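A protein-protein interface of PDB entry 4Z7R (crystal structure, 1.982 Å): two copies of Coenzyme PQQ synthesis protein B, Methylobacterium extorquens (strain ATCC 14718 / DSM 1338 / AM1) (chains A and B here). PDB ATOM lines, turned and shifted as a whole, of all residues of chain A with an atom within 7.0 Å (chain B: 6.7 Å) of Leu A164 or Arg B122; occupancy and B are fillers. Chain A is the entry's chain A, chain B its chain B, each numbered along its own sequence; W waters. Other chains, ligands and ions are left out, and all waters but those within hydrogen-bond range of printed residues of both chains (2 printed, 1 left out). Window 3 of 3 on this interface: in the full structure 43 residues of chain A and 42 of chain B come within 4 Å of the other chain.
Asn A121 touches Asn B121.
NH2 of Arg B122 touches O of Trp A163, 3.6 Å away.
Val B123 touches Trp A163.
CB of Trp A163 touches CG1 of Val B126, at 3.8 Å.
CD2 of Leu A164 touches CZ of Arg B122 (3.9 Å).
Water W1 bridges NH2 of Arg A122 (2.7 Å) and OD2 of Asp B120 (3.4 Å).
Water W2 lies within hydrogen-bond range of the backbone carbonyl oxygen of Asp B120 (2.7 Å), the backbone carbonyl oxygen of Asp A120 (3.1 Å) and the backbone NH of Arg A122 (3.1 Å).
The side-chain amide oxygen (OD1) of Asn A121 sits at hydrogen-bond distance from the backbone NH (N) of Arg B122, 3.0 Å away.
OD1 of Asn A121 lies within hydrogen-bond range of N of Val B123, 3.0 Å away.
The guanidinium group of Arg A122 lies within salt-bridge range of the side-chain carboxylate of Asp B120, at 3.7 Å.
The backbone NH of Arg A122 is in hydrogen-bond range of the side-chain amide oxygen of Asn B121 (3.0 Å).
Printed residues of chain B within 4 Å of Asn A121: Asn B121, Arg B122 and Val B123.
Printed residues of chain B within 4 Å of Trp A163: Arg B122 (3.6 Å), Val B123 (3.6 Å) and Val B126 (3.8 Å).
Leu A164 touches just one residue of chain B: Arg B122 (3.9 Å).
Printed residues of chain A within 4 Å of Asp B120: Arg A122 (3.4 Å).
Of the printed residues of chain A, Asn B121 touches Asn A121 (3.3 Å) and Arg A122 (3.0 Å).
Arg B122 touches three residues of chain A.
Phe B124 touches none of the printed residues of chain A.
Printed residues of chain A within 4 Å of Val B126: Trp A163 (3.8 Å).
The nearest residue of chain B that does not touch Leu A164 is Asp B125 (6.6 Å).
The nearest residue of chain A that does not touch Arg B122 is Glu A165 (5.0 Å).
The nearest printed residue of chain B that does not touch Arg A122 is Arg B122 (7.0 Å).
The indole nitrogen of Trp A163 is in hydrogen-bond range of the backbone carbonyl oxygen of Gly A89 (2.8 Å).
The side-chain amide nitrogen (ND2) of Asn A121 sits at hydrogen-bond distance from the backbone carbonyl oxygen (O) of Ser A117, at 2.9 Å.
Of the 9 printed residues of chain B, 5 touch a printed residue of chain A.
Hydrophobic or aromatic side chains of chain B that line the printed part of chain A: Val B123 and Val B126.
Hydrophobic or aromatic side chains of chain A within 4 Å of the printed part of chain B: Trp A163 and Leu A164.
Along chain A the printed residues that touch a printed residue of chain B span positions 121 to 164.
Among the printed residues, Asp or Glu carboxylates within 4 Å of a Lys or Arg side-chain nitrogen of the other chain: Arg A122 with Asp B120.
Asn A121 touches its own counterpart, Asn B121.
Asn A121 touches Arg B122, and with the chains exchanged Arg A122 touches Asn B121.
Arg A122 touches Asp B120, but with the chains exchanged Asp A120 does not touch Arg B122 (5.9 Å).
Positions printed for both chains: 120, 121 and 122.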
ATOM      1  N   GLY A  89      20.361   1.991  -6.608  1.00  0.00           N
ATOM      2  CA  GLY A  89      19.531   1.286  -5.648  1.00  0.00           C
ATOM      3  C   GLY A  89      19.450   1.904  -4.261  1.00  0.00           C
ATOM      4  O   GLY A  89      18.984   1.256  -3.324  1.00  0.00           O
ATOM      5  N   GLY A 113      20.946  -5.560 -12.581  1.00  0.00           N
ATOM      6  CA  GLY A 113      21.392  -5.636 -11.202  1.00  0.00           C
ATOM      7  C   GLY A 113      20.505  -4.879 -10.228  1.00  0.00           C
ATOM      8  O   GLY A 113      20.177  -5.385  -9.153  1.00  0.00           O
ATOM      9  N   ILE A 114      20.105  -3.669 -10.604  1.00  0.00           N
ATOM     10  CA  ILE A 114      19.286  -2.833  -9.731  1.00  0.00           C
ATOM     11  C   ILE A 114      17.853  -3.356  -9.613  1.00  0.00           C
ATOM     12  O   ILE A 114      17.320  -3.455  -8.507  1.00  0.00           O
ATOM     13  CB  ILE A 114      19.271  -1.369 -10.214  1.00  0.00           C
ATOM     14  CG1 ILE A 114      20.635  -0.732  -9.956  1.00  0.00           C
ATOM     15  CG2 ILE A 114      18.205  -0.568  -9.484  1.00  0.00           C
ATOM     16  CD1 ILE A 114      21.077  -0.821  -8.501  1.00  0.00           C
ATOM     17  N   SER A 117      17.820  -6.360  -7.382  1.00  0.00           N
ATOM     18  CA  SER A 117      17.955  -5.992  -5.976  1.00  0.00           C
ATOM     19  C   SER A 117      16.631  -5.490  -5.408  1.00  0.00           C
ATOM     20  O   SER A 117      16.258  -5.829  -4.284  1.00  0.00           O
ATOM     21  CB  SER A 117      19.042  -4.930  -5.796  1.00  0.00           C
ATOM     22  OG  SER A 117      20.327  -5.465  -6.059  1.00  0.00           O
ATOM     23  N   ASP A 120      14.066  -8.355  -5.244  1.00  0.00           N
ATOM     24  CA  ASP A 120      14.407  -9.303  -4.180  1.00  0.00           C
ATOM     25  C   ASP A 120      13.776  -8.897  -2.852  1.00  0.00           C
ATOM     26  O   ASP A 120      13.792  -9.664  -1.891  1.00  0.00           O
ATOM     27  CB  ASP A 120      15.924  -9.431  -4.017  1.00  0.00           C
ATOM     28  CG  ASP A 120      16.561 -10.249  -5.122  1.00  0.00           C
ATOM     29  OD1 ASP A 120      15.849 -11.062  -5.747  1.00  0.00           O
ATOM     30  OD2 ASP A 120      17.776 -10.083  -5.360  1.00  0.00           O
ATOM     31  N   ASN A 121      13.227  -7.688  -2.807  1.00  0.00           N
ATOM     32  CA  ASN A 121      12.482  -7.218  -1.645  1.00  0.00           C
ATOM     33  C   ASN A 121      10.984  -7.349  -1.902  1.00  0.00           C
ATOM     34  O   ASN A 121      10.418  -6.613  -2.708  1.00  0.00           O
ATOM     35  CB  ASN A 121      12.828  -5.764  -1.318  1.00  0.00           C
ATOM     36  CG  ASN A 121      14.232  -5.601  -0.773  1.00  0.00           C
ATOM     37  OD1 ASN A 121      14.451  -5.668   0.436  1.00  0.00           O
ATOM     38  ND2 ASN A 121      15.194  -5.378  -1.663  1.00  0.00           N
ATOM     39  N   ARG A 122      10.350  -8.294  -1.215  1.00  0.00           N
ATOM     40  CA  ARG A 122       8.933  -8.583  -1.421  1.00  0.00           C
ATOM     41  C   ARG A 122       8.014  -7.408  -1.083  1.00  0.00           C
ATOM     42  O   ARG A 122       6.870  -7.364  -1.532  1.00  0.00           O
ATOM     43  CB  ARG A 122       8.528  -9.818  -0.613  1.00  0.00           C
ATOM     44  CG  ARG A 122       8.990 -11.124  -1.243  1.00  0.00           C
ATOM     45  CD  ARG A 122       8.383 -12.328  -0.547  1.00  0.00           C
ATOM     46  NE  ARG A 122       8.853 -12.449   0.828  1.00  0.00           N
ATOM     47  CZ  ARG A 122      10.011 -13.002   1.173  1.00  0.00           C
ATOM     48  NH1 ARG A 122      10.823 -13.482   0.241  1.00  0.00           N
ATOM     49  NH2 ARG A 122      10.362 -13.072   2.450  1.00  0.00           N
ATOM     50  N   VAL A 160      28.246   1.022  -3.870  1.00  0.00           N
ATOM     51  CA  VAL A 160      27.063   0.194  -3.684  1.00  0.00           C
ATOM     52  C   VAL A 160      26.224   0.824  -2.574  1.00  0.00           C
ATOM     53  O   VAL A 160      26.772   1.449  -1.663  1.00  0.00           O
ATOM     54  CB  VAL A 160      27.423  -1.275  -3.347  1.00  0.00           C
ATOM     55  CG1 VAL A 160      28.528  -1.771  -4.266  1.00  0.00           C
ATOM     56  CG2 VAL A 160      27.837  -1.422  -1.891  1.00  0.00           C
ATOM     57  N   PRO A 161      24.891   0.697  -2.668  1.00  0.00           N
ATOM     58  CA  PRO A 161      23.992   1.287  -1.670  1.00  0.00           C
ATOM     59  C   PRO A 161      24.327   0.843  -0.253  1.00  0.00           C
ATOM     60  O   PRO A 161      24.857  -0.254  -0.062  1.00  0.00           O
ATOM     61  CB  PRO A 161      22.612   0.771  -2.089  1.00  0.00           C
ATOM     62  CG  PRO A 161      22.738   0.514  -3.544  1.00  0.00           C
ATOM     63  CD  PRO A 161      24.147   0.040  -3.757  1.00  0.00           C
ATOM     64  N   LEU A 162      24.021   1.698   0.718  1.00  0.00           N
ATOM     65  CA  LEU A 162      24.324   1.429   2.117  1.00  0.00           C
ATOM     66  C   LEU A 162      23.770   0.083   2.568  1.00  0.00           C
ATOM     67  O   LEU A 162      24.455  -0.673   3.256  1.00  0.00           O
ATOM     68  CB  LEU A 162      23.770   2.548   3.004  1.00  0.00           C
ATOM     69  CG  LEU A 162      24.772   3.247   3.925  1.00  0.00           C
ATOM     70  CD1 LEU A 162      25.991   3.693   3.138  1.00  0.00           C
ATOM     71  CD2 LEU A 162      24.115   4.436   4.610  1.00  0.00           C
ATOM     72  N   TRP A 163      22.541  -0.227   2.159  1.00  0.00           N
ATOM     73  CA  TRP A 163      21.885  -1.454   2.609  1.00  0.00           C
ATOM     74  C   TRP A 163      22.405  -2.698   1.890  1.00  0.00           C
ATOM     75  O   TRP A 163      21.935  -3.807   2.145  1.00  0.00           O
ATOM     76  CB  TRP A 163      20.359  -1.350   2.452  1.00  0.00           C
ATOM     77  CG  TRP A 163      19.854  -1.064   1.064  1.00  0.00           C
ATOM     78  CD1 TRP A 163      19.782   0.156   0.451  1.00  0.00           C
ATOM     79  CD2 TRP A 163      19.311  -2.011   0.134  1.00  0.00           C
ATOM     80  NE1 TRP A 163      19.247   0.022  -0.808  1.00  0.00           N
ATOM     81  CE2 TRP A 163      18.947  -1.297  -1.027  1.00  0.00           C
ATOM     82  CE3 TRP A 163      19.105  -3.395   0.165  1.00  0.00           C
ATOM     83  CZ2 TRP A 163      18.392  -1.919  -2.144  1.00  0.00           C
ATOM     84  CZ3 TRP A 163      18.550  -4.011  -0.944  1.00  0.00           C
ATOM     85  CH2 TRP A 163      18.203  -3.274  -2.084  1.00  0.00           C
ATOM     86  N   LEU A 164      23.380  -2.513   1.005  1.00  0.00           N
ATOM     87  CA  LEU A 164      24.033  -3.634   0.331  1.00  0.00           C
ATOM     88  C   LEU A 164      25.543  -3.623   0.563  1.00  0.00           C
ATOM     89  O   LEU A 164      26.279  -4.396  -0.051  1.00  0.00           O
ATOM     90  CB  LEU A 164      23.739  -3.610  -1.171  1.00  0.00           C
ATOM     91  CG  LEU A 164      22.302  -3.886  -1.620  1.00  0.00           C
ATOM     92  CD1 LEU A 164      22.183  -3.733  -3.126  1.00  0.00           C
ATOM     93  CD2 LEU A 164      21.858  -5.275  -1.186  1.00  0.00           C
ATOM     94  N   GLU A 165      26.001  -2.739   1.446  1.00  0.00           N
ATOM     95  CA  GLU A 165      27.429  -2.611   1.728  1.00  0.00           C
ATOM     96  C   GLU A 165      27.977  -3.850   2.421  1.00  0.00           C
ATOM     97  O   GLU A 165      27.309  -4.448   3.263  1.00  0.00           O
ATOM     98  CB  GLU A 165      27.706  -1.377   2.587  1.00  0.00           C
ATOM     99  CG  GLU A 165      27.780  -0.078   1.809  1.00  0.00           C
ATOM    100  CD  GLU A 165      28.377   1.050   2.627  1.00  0.00           C
ATOM    101  OE1 GLU A 165      28.621   0.844   3.834  1.00  0.00           O
ATOM    102  OE2 GLU A 165      28.607   2.139   2.062  1.00  0.00           O
ATOM    103  N   ASP A 166      29.202  -4.224   2.072  1.00  0.00           N
ATOM    104  CA  ASP A 166      29.794  -5.438   2.613  1.00  0.00           C
ATOM    105  C   ASP A 166      31.279  -5.267   2.951  1.00  0.00           C
ATOM    106  O   ASP A 166      31.843  -4.188   2.769  1.00  0.00           O
ATOM    107  CB  ASP A 166      29.579  -6.595   1.629  1.00  0.00           C
ATOM    108  CG  ASP A 166      30.268  -6.380   0.283  1.00  0.00           C
ATOM    109  OD1 ASP A 166      31.465  -6.030   0.254  1.00  0.00           O
ATOM    110  OD2 ASP A 166      29.608  -6.592  -0.757  1.00  0.00           O
ATOM    111  N   ALA A 167      31.905  -6.339   3.433  1.00  0.00           N
ATOM    112  CA  ALA A 167      33.283  -6.282   3.926  1.00  0.00           C
ATOM    113  C   ALA A 167      34.304  -6.060   2.815  1.00  0.00           C
ATOM    114  O   ALA A 167      35.444  -5.675   3.077  1.00  0.00           O
ATOM    115  CB  ALA A 167      33.618  -7.554   4.694  1.00  0.00           C
ATOM    116  N   MET A 169      33.720  -3.906   0.271  1.00  0.00           N
ATOM    117  CA  MET A 169      32.890  -2.868  -0.332  1.00  0.00           C
ATOM    118  C   MET A 169      33.468  -2.280  -1.610  1.00  0.00           C
ATOM    119  O   MET A 169      34.671  -2.034  -1.716  1.00  0.00           O
ATOM    120  CB  MET A 169      32.643  -1.738   0.668  1.00  0.00           C
ATOM    121  CG  MET A 169      31.382  -0.938   0.383  1.00  0.00           C
ATOM    122  SD  MET A 169      31.456   0.745   1.019  1.00  0.00           S
ATOM    123  CE  MET A 169      32.488   0.517   2.465  1.00  0.00           C
ATOM    124  N   THR A 177      25.517  -1.080 -11.145  1.00  0.00           N
ATOM    125  CA  THR A 177      25.009  -0.608  -9.861  1.00  0.00           C
ATOM    126  C   THR A 177      24.720   0.895  -9.865  1.00  0.00           C
ATOM    127  O   THR A 177      23.771   1.350  -9.232  1.00  0.00           O
ATOM    128  CB  THR A 177      26.005  -0.945  -8.727  1.00  0.00           C
ATOM    129  OG1 THR A 177      26.182  -2.364  -8.662  1.00  0.00           O
ATOM    130  CG2 THR A 177      25.500  -0.445  -7.383  1.00  0.00           C
ATOM    131  N   VAL B 118       9.760  -7.777   8.067  1.00  0.00           N
ATOM    132  CA  VAL B 118      10.637  -6.629   7.869  1.00  0.00           C
ATOM    133  C   VAL B 118      12.065  -7.100   7.611  1.00  0.00           C
ATOM    134  O   VAL B 118      12.700  -6.685   6.640  1.00  0.00           O
ATOM    135  CB  VAL B 118      10.614  -5.676   9.081  1.00  0.00           C
ATOM    136  CG1 VAL B 118      11.682  -4.605   8.935  1.00  0.00           C
ATOM    137  CG2 VAL B 118       9.239  -5.042   9.230  1.00  0.00           C
ATOM    138  N   SER B 119      12.567  -7.965   8.489  1.00  0.00           N
ATOM    139  CA  SER B 119      13.917  -8.504   8.349  1.00  0.00           C
ATOM    140  C   SER B 119      14.098  -9.291   7.051  1.00  0.00           C
ATOM    141  O   SER B 119      15.221  -9.450   6.573  1.00  0.00           O
ATOM    142  CB  SER B 119      14.259  -9.399   9.543  1.00  0.00           C
ATOM    143  OG  SER B 119      13.475 -10.580   9.535  1.00  0.00           O
ATOM    144  N   ASP B 120      12.998  -9.778   6.481  1.00  0.00           N
ATOM    145  CA  ASP B 120      13.058 -10.497   5.209  1.00  0.00           C
ATOM    146  C   ASP B 120      13.302  -9.560   4.029  1.00  0.00           C
ATOM    147  O   ASP B 120      13.601 -10.010   2.923  1.00  0.00           O
ATOM    148  CB  ASP B 120      11.768 -11.288   4.978  1.00  0.00           C
ATOM    149  CG  ASP B 120      11.674 -12.522   5.853  1.00  0.00           C
ATOM    150  OD1 ASP B 120      12.730 -13.019   6.298  1.00  0.00           O
ATOM    151  OD2 ASP B 120      10.543 -12.992   6.098  1.00  0.00           O
ATOM    152  N   ASN B 121      13.149  -8.260   4.264  1.00  0.00           N
ATOM    153  CA  ASN B 121      13.476  -7.250   3.262  1.00  0.00           C
ATOM    154  C   ASN B 121      14.793  -6.551   3.594  1.00  0.00           C
ATOM    155  O   ASN B 121      14.862  -5.779   4.553  1.00  0.00           O
ATOM    156  CB  ASN B 121      12.346  -6.225   3.151  1.00  0.00           C
ATOM    157  CG  ASN B 121      11.088  -6.805   2.527  1.00  0.00           C
ATOM    158  OD1 ASN B 121      10.911  -6.771   1.312  1.00  0.00           O
ATOM    159  ND2 ASN B 121      10.203  -7.341   3.365  1.00  0.00           N
ATOM    160  N   ARG B 122      15.839  -6.821   2.818  1.00  0.00           N
ATOM    161  CA  ARG B 122      17.150  -6.244   3.109  1.00  0.00           C
ATOM    162  C   ARG B 122      17.177  -4.719   3.004  1.00  0.00           C
ATOM    163  O   ARG B 122      18.049  -4.075   3.581  1.00  0.00           O
ATOM    164  CB  ARG B 122      18.227  -6.834   2.194  1.00  0.00           C
ATOM    165  CG  ARG B 122      18.682  -8.233   2.583  1.00  0.00           C
ATOM    166  CD  ARG B 122      19.927  -8.633   1.810  1.00  0.00           C
ATOM    167  NE  ARG B 122      21.084  -7.837   2.217  1.00  0.00           N
ATOM    168  CZ  ARG B 122      22.295  -7.940   1.678  1.00  0.00           C
ATOM    169  NH1 ARG B 122      22.518  -8.805   0.698  1.00  0.00           N
ATOM    170  NH2 ARG B 122      23.284  -7.174   2.117  1.00  0.00           N
ATOM    171  N   VAL B 123      16.232  -4.136   2.273  1.00  0.00           N
ATOM    172  CA  VAL B 123      16.185  -2.682   2.148  1.00  0.00           C
ATOM    173  C   VAL B 123      15.924  -2.015   3.510  1.00  0.00           C
ATOM    174  O   VAL B 123      16.340  -0.880   3.745  1.00  0.00           O
ATOM    175  CB  VAL B 123      15.118  -2.236   1.118  1.00  0.00           C
ATOM    176  CG1 VAL B 123      13.706  -2.503   1.629  1.00  0.00           C
ATOM    177  CG2 VAL B 123      15.302  -0.769   0.759  1.00  0.00           C
ATOM    178  N   PHE B 124      15.261  -2.729   4.414  1.00  0.00           N
ATOM    179  CA  PHE B 124      15.018  -2.206   5.755  1.00  0.00           C
ATOM    180  C   PHE B 124      16.234  -2.339   6.673  1.00  0.00           C
ATOM    181  O   PHE B 124      16.172  -1.966   7.846  1.00  0.00           O
ATOM    182  CB  PHE B 124      13.808  -2.895   6.392  1.00  0.00           C
ATOM    183  CG  PHE B 124      12.491  -2.476   5.799  1.00  0.00           C
ATOM    184  CD1 PHE B 124      11.912  -1.269   6.154  1.00  0.00           C
ATOM    185  CD2 PHE B 124      11.828  -3.290   4.899  1.00  0.00           C
ATOM    186  CE1 PHE B 124      10.701  -0.877   5.615  1.00  0.00           C
ATOM    187  CE2 PHE B 124      10.615  -2.906   4.356  1.00  0.00           C
ATOM    188  CZ  PHE B 124      10.051  -1.698   4.714  1.00  0.00           C
ATOM    189  N   ASP B 125      17.333  -2.877   6.150  1.00  0.00           N
ATOM    190  CA  ASP B 125      18.590  -2.908   6.901  1.00  0.00           C
ATOM    191  C   ASP B 125      19.206  -1.517   7.048  1.00  0.00           C
ATOM    192  O   ASP B 125      20.229  -1.357   7.710  1.00  0.00           O
ATOM    193  CB  ASP B 125      19.604  -3.856   6.255  1.00  0.00           C
ATOM    194  CG  ASP B 125      19.217  -5.315   6.405  1.00  0.00           C
ATOM    195  OD1 ASP B 125      18.222  -5.603   7.104  1.00  0.00           O
ATOM    196  OD2 ASP B 125      19.919  -6.173   5.834  1.00  0.00           O
ATOM    197  N   VAL B 126      18.599  -0.514   6.414  1.00  0.00           N
ATOM    198  CA  VAL B 126      19.024   0.867   6.619  1.00  0.00           C
ATOM    199  C   VAL B 126      18.813   1.273   8.079  1.00  0.00           C
ATOM    200  O   VAL B 126      19.430   2.220   8.565  1.00  0.00           O
ATOM    201  CB  VAL B 126      18.279   1.840   5.687  1.00  0.00           C
ATOM    202  CG1 VAL B 126      18.601   1.528   4.231  1.00  0.00           C
ATOM    203  CG2 VAL B 126      16.779   1.787   5.941  1.00  0.00           C
HETATM  204  O   HOH W   1       8.373 -11.826   3.696  1.00  0.00           O
HETATM  205  O   HOH W   2      12.116 -10.046   0.692  1.00  0.00           O
